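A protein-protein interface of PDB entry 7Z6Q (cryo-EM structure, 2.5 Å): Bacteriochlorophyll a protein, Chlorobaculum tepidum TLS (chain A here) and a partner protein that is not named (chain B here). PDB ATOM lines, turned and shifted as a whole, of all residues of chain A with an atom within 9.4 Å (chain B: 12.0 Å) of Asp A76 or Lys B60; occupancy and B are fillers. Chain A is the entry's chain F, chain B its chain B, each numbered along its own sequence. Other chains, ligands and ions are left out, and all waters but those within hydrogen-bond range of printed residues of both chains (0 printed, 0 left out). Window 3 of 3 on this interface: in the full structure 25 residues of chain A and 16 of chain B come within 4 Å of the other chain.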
ATOM      1  N   SER A  42      13.706  -4.323   0.299  1.00  0.00           N
ATOM      2  CA  SER A  42      13.543  -4.308  -1.147  1.00  0.00           C
ATOM      3  C   SER A  42      14.556  -5.244  -1.800  1.00  0.00           C
ATOM      4  O   SER A  42      15.764  -5.113  -1.555  1.00  0.00           O
ATOM      5  CB  SER A  42      13.715  -2.890  -1.688  1.00  0.00           C
ATOM      6  OG  SER A  42      14.052  -2.910  -3.064  1.00  0.00           O
ATOM      7  N   PRO A  43      14.115  -6.194  -2.630  1.00  0.00           N
ATOM      8  CA  PRO A  43      15.057  -7.092  -3.304  1.00  0.00           C
ATOM      9  C   PRO A  43      15.808  -6.454  -4.462  1.00  0.00           C
ATOM     10  O   PRO A  43      16.602  -7.142  -5.112  1.00  0.00           O
ATOM     11  CB  PRO A  43      14.154  -8.231  -3.794  1.00  0.00           C
ATOM     12  CG  PRO A  43      12.820  -7.621  -3.947  1.00  0.00           C
ATOM     13  CD  PRO A  43      12.713  -6.502  -2.951  1.00  0.00           C
ATOM     14  N   LEU A  44      15.568  -5.178  -4.750  1.00  0.00           N
ATOM     15  CA  LEU A  44      16.404  -4.397  -5.651  1.00  0.00           C
ATOM     16  C   LEU A  44      16.875  -3.145  -4.931  1.00  0.00           C
ATOM     17  O   LEU A  44      16.063  -2.402  -4.371  1.00  0.00           O
ATOM     18  CB  LEU A  44      15.669  -4.011  -6.935  1.00  0.00           C
ATOM     19  CG  LEU A  44      15.280  -5.132  -7.890  1.00  0.00           C
ATOM     20  CD1 LEU A  44      14.531  -4.549  -9.073  1.00  0.00           C
ATOM     21  CD2 LEU A  44      16.516  -5.890  -8.340  1.00  0.00           C
ATOM     22  N   LEU A  45      18.188  -2.929  -5.011  1.00  0.00           N
ATOM     23  CA  LEU A  45      18.860  -1.742  -4.430  1.00  0.00           C
ATOM     24  C   LEU A  45      19.874  -1.228  -5.457  1.00  0.00           C
ATOM     25  O   LEU A  45      20.278  -2.018  -6.332  1.00  0.00           O
ATOM     26  CB  LEU A  45      19.520  -2.131  -3.105  1.00  0.00           C
ATOM     27  CG  LEU A  45      18.561  -2.640  -2.032  1.00  0.00           C
ATOM     28  CD1 LEU A  45      19.313  -3.141  -0.813  1.00  0.00           C
ATOM     29  CD2 LEU A  45      17.562  -1.563  -1.647  1.00  0.00           C
ATOM     30  N   PRO A  46      20.293   0.055  -5.417  1.00  0.00           N
ATOM     31  CA  PRO A  46      19.652   1.074  -4.581  1.00  0.00           C
ATOM     32  C   PRO A  46      18.284   1.527  -5.109  1.00  0.00           C
ATOM     33  O   PRO A  46      18.090   1.513  -6.302  1.00  0.00           O
ATOM     34  CB  PRO A  46      20.609   2.273  -4.646  1.00  0.00           C
ATOM     35  CG  PRO A  46      21.862   1.748  -5.312  1.00  0.00           C
ATOM     36  CD  PRO A  46      21.412   0.595  -6.180  1.00  0.00           C
ATOM     37  N   ALA A  47      17.361   1.865  -4.209  1.00  0.00           N
ATOM     38  CA  ALA A  47      16.042   2.382  -4.631  1.00  0.00           C
ATOM     39  C   ALA A  47      15.817   3.725  -3.937  1.00  0.00           C
ATOM     40  O   ALA A  47      15.724   3.731  -2.704  1.00  0.00           O
ATOM     41  CB  ALA A  47      14.966   1.387  -4.278  1.00  0.00           C
ATOM     42  N   ASP A  48      15.685   4.809  -4.703  1.00  0.00           N
ATOM     43  CA  ASP A  48      15.490   6.153  -4.097  1.00  0.00           C
ATOM     44  C   ASP A  48      14.108   6.679  -4.484  1.00  0.00           C
ATOM     45  O   ASP A  48      13.544   6.147  -5.452  1.00  0.00           O
ATOM     46  CB  ASP A  48      16.584   7.131  -4.534  1.00  0.00           C
ATOM     47  CG  ASP A  48      17.940   6.869  -3.903  1.00  0.00           C
ATOM     48  OD1 ASP A  48      18.088   5.816  -3.259  1.00  0.00           O
ATOM     49  OD2 ASP A  48      18.831   7.725  -4.045  1.00  0.00           O
ATOM     50  N   SER A  73      11.038   8.294  -8.670  1.00  0.00           N
ATOM     51  CA  SER A  73      11.830   7.250  -7.978  1.00  0.00           C
ATOM     52  C   SER A  73      12.765   6.537  -8.954  1.00  0.00           C
ATOM     53  O   SER A  73      12.304   6.144 -10.030  1.00  0.00           O
ATOM     54  CB  SER A  73      10.917   6.260  -7.305  1.00  0.00           C
ATOM     55  OG  SER A  73      10.500   5.249  -8.212  1.00  0.00           O
ATOM     56  N   ILE A  74      14.028   6.360  -8.570  1.00  0.00           N
ATOM     57  CA  ILE A  74      14.968   5.575  -9.417  1.00  0.00           C
ATOM     58  C   ILE A  74      15.120   4.232  -8.707  1.00  0.00           C
ATOM     59  O   ILE A  74      15.558   4.226  -7.549  1.00  0.00           O
ATOM     60  CB  ILE A  74      16.323   6.291  -9.578  1.00  0.00           C
ATOM     61  CG1 ILE A  74      16.147   7.732 -10.063  1.00  0.00           C
ATOM     62  CG2 ILE A  74      17.245   5.496 -10.491  1.00  0.00           C
ATOM     63  CD1 ILE A  74      17.444   8.461 -10.305  1.00  0.00           C
ATOM     64  N   VAL A  75      14.719   3.153  -9.390  1.00  0.00           N
ATOM     65  CA  VAL A  75      14.776   1.770  -8.834  1.00  0.00           C
ATOM     66  C   VAL A  75      15.764   0.936  -9.658  1.00  0.00           C
ATOM     67  O   VAL A  75      15.469   0.647 -10.834  1.00  0.00           O
ATOM     68  CB  VAL A  75      13.382   1.116  -8.800  1.00  0.00           C
ATOM     69  CG1 VAL A  75      13.443  -0.321  -8.304  1.00  0.00           C
ATOM     70  CG2 VAL A  75      12.398   1.928  -7.970  1.00  0.00           C
ATOM     71  N   ASP A  76      16.896   0.587  -9.041  1.00  0.00           N
ATOM     72  CA  ASP A  76      17.970  -0.239  -9.661  1.00  0.00           C
ATOM     73  C   ASP A  76      18.357   0.384 -11.007  1.00  0.00           C
ATOM     74  O   ASP A  76      18.413  -0.356 -12.009  1.00  0.00           O
ATOM     75  CB  ASP A  76      17.601  -1.721  -9.760  1.00  0.00           C
ATOM     76  CG  ASP A  76      18.722  -2.588 -10.307  1.00  0.00           C
ATOM     77  OD1 ASP A  76      19.777  -2.033 -10.658  1.00  0.00           O
ATOM     78  OD2 ASP A  76      18.533  -3.815 -10.372  1.00  0.00           O
ATOM     79  N   SER A  77      18.595   1.705 -10.996  1.00  0.00           N
ATOM     80  CA  SER A  77      18.987   2.557 -12.157  1.00  0.00           C
ATOM     81  C   SER A  77      17.840   2.715 -13.168  1.00  0.00           C
ATOM     82  O   SER A  77      18.100   3.246 -14.265  1.00  0.00           O
ATOM     83  CB  SER A  77      20.282   2.118 -12.810  1.00  0.00           C
ATOM     84  OG  SER A  77      20.072   0.998 -13.659  1.00  0.00           O
ATOM     85  N   THR A  78      16.618   2.312 -12.800  1.00  0.00           N
ATOM     86  CA  THR A  78      15.448   2.463 -13.701  1.00  0.00           C
ATOM     87  C   THR A  78      14.568   3.642 -13.292  1.00  0.00           C
ATOM     88  O   THR A  78      13.896   3.535 -12.257  1.00  0.00           O
ATOM     89  CB  THR A  78      14.698   1.126 -13.713  1.00  0.00           C
ATOM     90  OG1 THR A  78      15.589   0.132 -14.218  1.00  0.00           O
ATOM     91  CG2 THR A  78      13.450   1.161 -14.565  1.00  0.00           C
ATOM     92  N   LYS A  79      14.609   4.735 -14.054  1.00  0.00           N
ATOM     93  CA  LYS A  79      13.799   5.918 -13.675  1.00  0.00           C
ATOM     94  C   LYS A  79      12.324   5.517 -13.729  1.00  0.00           C
ATOM     95  O   LYS A  79      11.899   4.963 -14.753  1.00  0.00           O
ATOM     96  CB  LYS A  79      14.079   7.070 -14.645  1.00  0.00           C
ATOM     97  CG  LYS A  79      15.482   7.654 -14.580  1.00  0.00           C
ATOM     98  CD  LYS A  79      15.714   8.771 -15.572  1.00  0.00           C
ATOM     99  CE  LYS A  79      17.104   9.363 -15.485  1.00  0.00           C
ATOM    100  NZ  LYS A  79      17.302  10.438 -16.488  1.00  0.00           N
ATOM    101  N   ASN A  80      11.582   5.805 -12.660  1.00  0.00           N
ATOM    102  CA  ASN A  80      10.133   5.489 -12.600  1.00  0.00           C
ATOM    103  C   ASN A  80       9.408   6.763 -12.166  1.00  0.00           C
ATOM    104  O   ASN A  80       9.821   7.344 -11.154  1.00  0.00           O
ATOM    105  CB  ASN A  80       9.841   4.368 -11.600  1.00  0.00           C
ATOM    106  CG  ASN A  80      10.587   3.085 -11.892  1.00  0.00           C
ATOM    107  OD1 ASN A  80      10.844   2.758 -13.044  1.00  0.00           O
ATOM    108  ND2 ASN A  80      10.919   2.339 -10.853  1.00  0.00           N
ATOM    109  N   SER A 260      17.655   4.799  -0.391  1.00  0.00           N
ATOM    110  CA  SER A 260      17.869   3.452   0.196  1.00  0.00           C
ATOM    111  C   SER A 260      18.861   2.636  -0.635  1.00  0.00           C
ATOM    112  O   SER A 260      18.921   2.848  -1.853  1.00  0.00           O
ATOM    113  CB  SER A 260      16.560   2.725   0.363  1.00  0.00           C
ATOM    114  OG  SER A 260      16.102   2.213  -0.878  1.00  0.00           O
ATOM    115  N   ASP A 261      19.610   1.764   0.045  1.00  0.00           N
ATOM    116  CA  ASP A 261      20.633   0.876  -0.566  1.00  0.00           C
ATOM    117  C   ASP A 261      21.110  -0.119   0.498  1.00  0.00           C
ATOM    118  O   ASP A 261      20.530  -0.143   1.606  1.00  0.00           O
ATOM    119  CB  ASP A 261      21.821   1.678  -1.105  1.00  0.00           C
ATOM    120  CG  ASP A 261      22.484   2.553  -0.056  1.00  0.00           C
ATOM    121  OD1 ASP A 261      21.925   2.662   1.054  1.00  0.00           O
ATOM    122  OD2 ASP A 261      23.554   3.118  -0.356  1.00  0.00           O
ATOM    123  N   SER A 262      22.139  -0.900   0.172  1.00  0.00           N
ATOM    124  CA  SER A 262      22.700  -1.888   1.132  1.00  0.00           C
ATOM    125  C   SER A 262      22.981  -1.261   2.508  1.00  0.00           C
ATOM    126  O   SER A 262      22.729  -1.932   3.517  1.00  0.00           O
ATOM    127  CB  SER A 262      23.944  -2.517   0.569  1.00  0.00           C
ATOM    128  OG  SER A 262      23.625  -3.391  -0.500  1.00  0.00           O
ATOM    129  N   LYS B  60      24.822   2.899 -11.625  1.00  0.00           N
ATOM    130  CA  LYS B  60      23.652   3.055 -10.720  1.00  0.00           C
ATOM    131  C   LYS B  60      23.417   4.543 -10.446  1.00  0.00           C
ATOM    132  O   LYS B  60      24.025   5.066  -9.497  1.00  0.00           O
ATOM    133  CB  LYS B  60      23.893   2.310  -9.404  1.00  0.00           C
ATOM    134  CG  LYS B  60      24.135   0.814  -9.541  1.00  0.00           C
ATOM    135  CD  LYS B  60      22.880  -0.017  -9.361  1.00  0.00           C
ATOM    136  CE  LYS B  60      23.175  -1.473  -9.072  1.00  0.00           C
ATOM    137  NZ  LYS B  60      21.934  -2.282  -8.996  1.00  0.00           N
ATOM    138  N   PRO B  61      22.557   5.241 -11.222  1.00  0.00           N
ATOM    139  CA  PRO B  61      22.276   6.663 -10.993  1.00  0.00           C
ATOM    140  C   PRO B  61      21.382   6.871  -9.761  1.00  0.00           C
ATOM    141  O   PRO B  61      20.752   5.933  -9.321  1.00  0.00           O
ATOM    142  CB  PRO B  61      21.531   7.088 -12.265  1.00  0.00           C
ATOM    143  CG  PRO B  61      22.077   6.168 -13.331  1.00  0.00           C
ATOM    144  CD  PRO B  61      22.261   4.832 -12.640  1.00  0.00           C
ATOM    145  N   ARG B  62      21.344   8.096  -9.235  1.00  0.00           N
ATOM    146  CA  ARG B  62      20.508   8.380  -8.040  1.00  0.00           C
ATOM    147  C   ARG B  62      19.888   9.774  -8.176  1.00  0.00           C
ATOM    148  O   ARG B  62      20.258  10.502  -9.114  1.00  0.00           O
ATOM    149  CB  ARG B  62      21.341   8.263  -6.760  1.00  0.00           C
ATOM    150  CG  ARG B  62      21.726   6.841  -6.380  1.00  0.00           C
ATOM    151  CD  ARG B  62      21.323   6.540  -4.952  1.00  0.00           C
ATOM    152  NE  ARG B  62      22.070   5.451  -4.345  1.00  0.00           N
ATOM    153  CZ  ARG B  62      21.882   5.025  -3.103  1.00  0.00           C
ATOM    154  NH1 ARG B  62      22.605   4.028  -2.623  1.00  0.00           N
ATOM    155  NH2 ARG B  62      20.966   5.601  -2.345  1.00  0.00           N
ATOM    156  N   LEU B  63      18.968  10.103  -7.268  1.00  0.00           N
ATOM    157  CA  LEU B  63      18.258  11.408  -7.220  1.00  0.00           C
ATOM    158  C   LEU B  63      19.088  12.396  -6.391  1.00  0.00           C
ATOM    159  O   LEU B  63      20.070  11.962  -5.755  1.00  0.00           O
ATOM    160  CB  LEU B  63      16.871  11.200  -6.605  1.00  0.00           C
ATOM    161  CG  LEU B  63      15.918  10.326  -7.418  1.00  0.00           C
ATOM    162  CD1 LEU B  63      14.631  10.066  -6.650  1.00  0.00           C
ATOM    163  CD2 LEU B  63      15.614  10.964  -8.765  1.00  0.00           C
ATOM    164  N   ALA B  64      18.691  13.671  -6.376  1.00  0.00           N
ATOM    165  CA  ALA B  64      19.462  14.686  -5.621  1.00  0.00           C
ATOM    166  C   ALA B  64      19.520  14.251  -4.152  1.00  0.00           C
ATOM    167  O   ALA B  64      18.475  13.865  -3.595  1.00  0.00           O
ATOM    168  CB  ALA B  64      18.820  16.043  -5.775  1.00  0.00           C
ATOM    169  N   SER B  65      20.706  14.353  -3.548  1.00  0.00           N
ATOM    170  CA  SER B  65      20.951  13.897  -2.154  1.00  0.00           C
ATOM    171  C   SER B  65      20.035  14.583  -1.134  1.00  0.00           C
ATOM    172  O   SER B  65      19.695  15.767  -1.317  1.00  0.00           O
ATOM    173  CB  SER B  65      22.398  14.079  -1.780  1.00  0.00           C
ATOM    174  OG  SER B  65      22.781  15.439  -1.913  1.00  0.00           O
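The side-chain carboxylate of Asp A76 lies within salt-bridge range of the side-chain amino group of Lys B60 (2.7 Å).
NH2 of Arg B62 lies within salt-bridge range of OD1 of Asp A48 (3.0 Å).
OD2 of Asp A261 lies within salt-bridge range of NH1 of Arg B62, 2.6 Å away.
The guanidinium group (NH2) of Arg B62 lies within hydrogen-bond range of the backbone carbonyl oxygen (O) of Ser A260, at 3.5 Å.
The side-chain amino group (NZ) of Lys B60 lies within hydrogen-bond range of the backbone carbonyl oxygen (O) of Leu A45, at 3.1 Å.
The backbone NH of Asp A48 sits at hydrogen-bond distance from the backbone carbonyl oxygen of Ile A74 (2.9 Å).
The backbone NH (N) of Asp A76 sits at hydrogen-bond distance from the backbone carbonyl oxygen (O) of Pro A46 (3.1 Å).
The side-chain carboxylate (OD1) of Asp A48 lies within hydrogen-bond range of the backbone NH (N) of Ser A260.
O of Ala A47 is in hydrogen-bond range of OG of Ser A260 (2.4 Å).
Among the printed residues, merely in contact across the chains: Pro A46 with Arg B62 (3.3 Å), Ser A77 with Pro B61 (3.4 Å), Ile A74 with Leu B63 (3.5 Å), Ile A74 with Arg B62 (3.5 Å), Pro A46 with Lys B60 (3.6 Å) and Ile A74 with Pro B61 (3.7 Å).
Ser A42 touches none of the printed residues of chain B.
Of the printed residues of chain B, Leu A45 touches Lys B60 (3.1 Å).
No residue of chain B comes within 4 Å of Ala A47.
Of the printed residues of chain B, Asp A48 touches Arg B62.
No residue of chain B comes within 4 Å of Val A75.
Asp A76 touches just one residue of chain B: Lys B60.
Ser A77 touches just one residue of chain B: Pro B61 (3.4 Å).
No residue of chain B comes within 4 Å of Thr A78.
Lys B60 touches three residues of chain A.
Printed residues of chain A within 4 Å of Leu B63: Ile A74 (3.5 Å).
The nearest residue of chain B that does not touch Asp A76 is Pro B61 (6.1 Å).
Of the 18 printed residues of chain A, 8 touch a printed residue of chain B.
Of the 6 printed residues of chain B, 4 touch a printed residue of chain A.
Hydrophobic or aromatic side chains of chain B that line the printed part of chain A: Pro B61 and Leu B63.
Among the printed residues, Asp or Glu carboxylates within 4 Å of a Lys or Arg side-chain nitrogen of the other chain: Asp A48 with Arg B62 (3.0 Å), Asp A76 with Lys B60 (2.7 Å) and Asp A261 with Arg B62 (2.6 Å).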
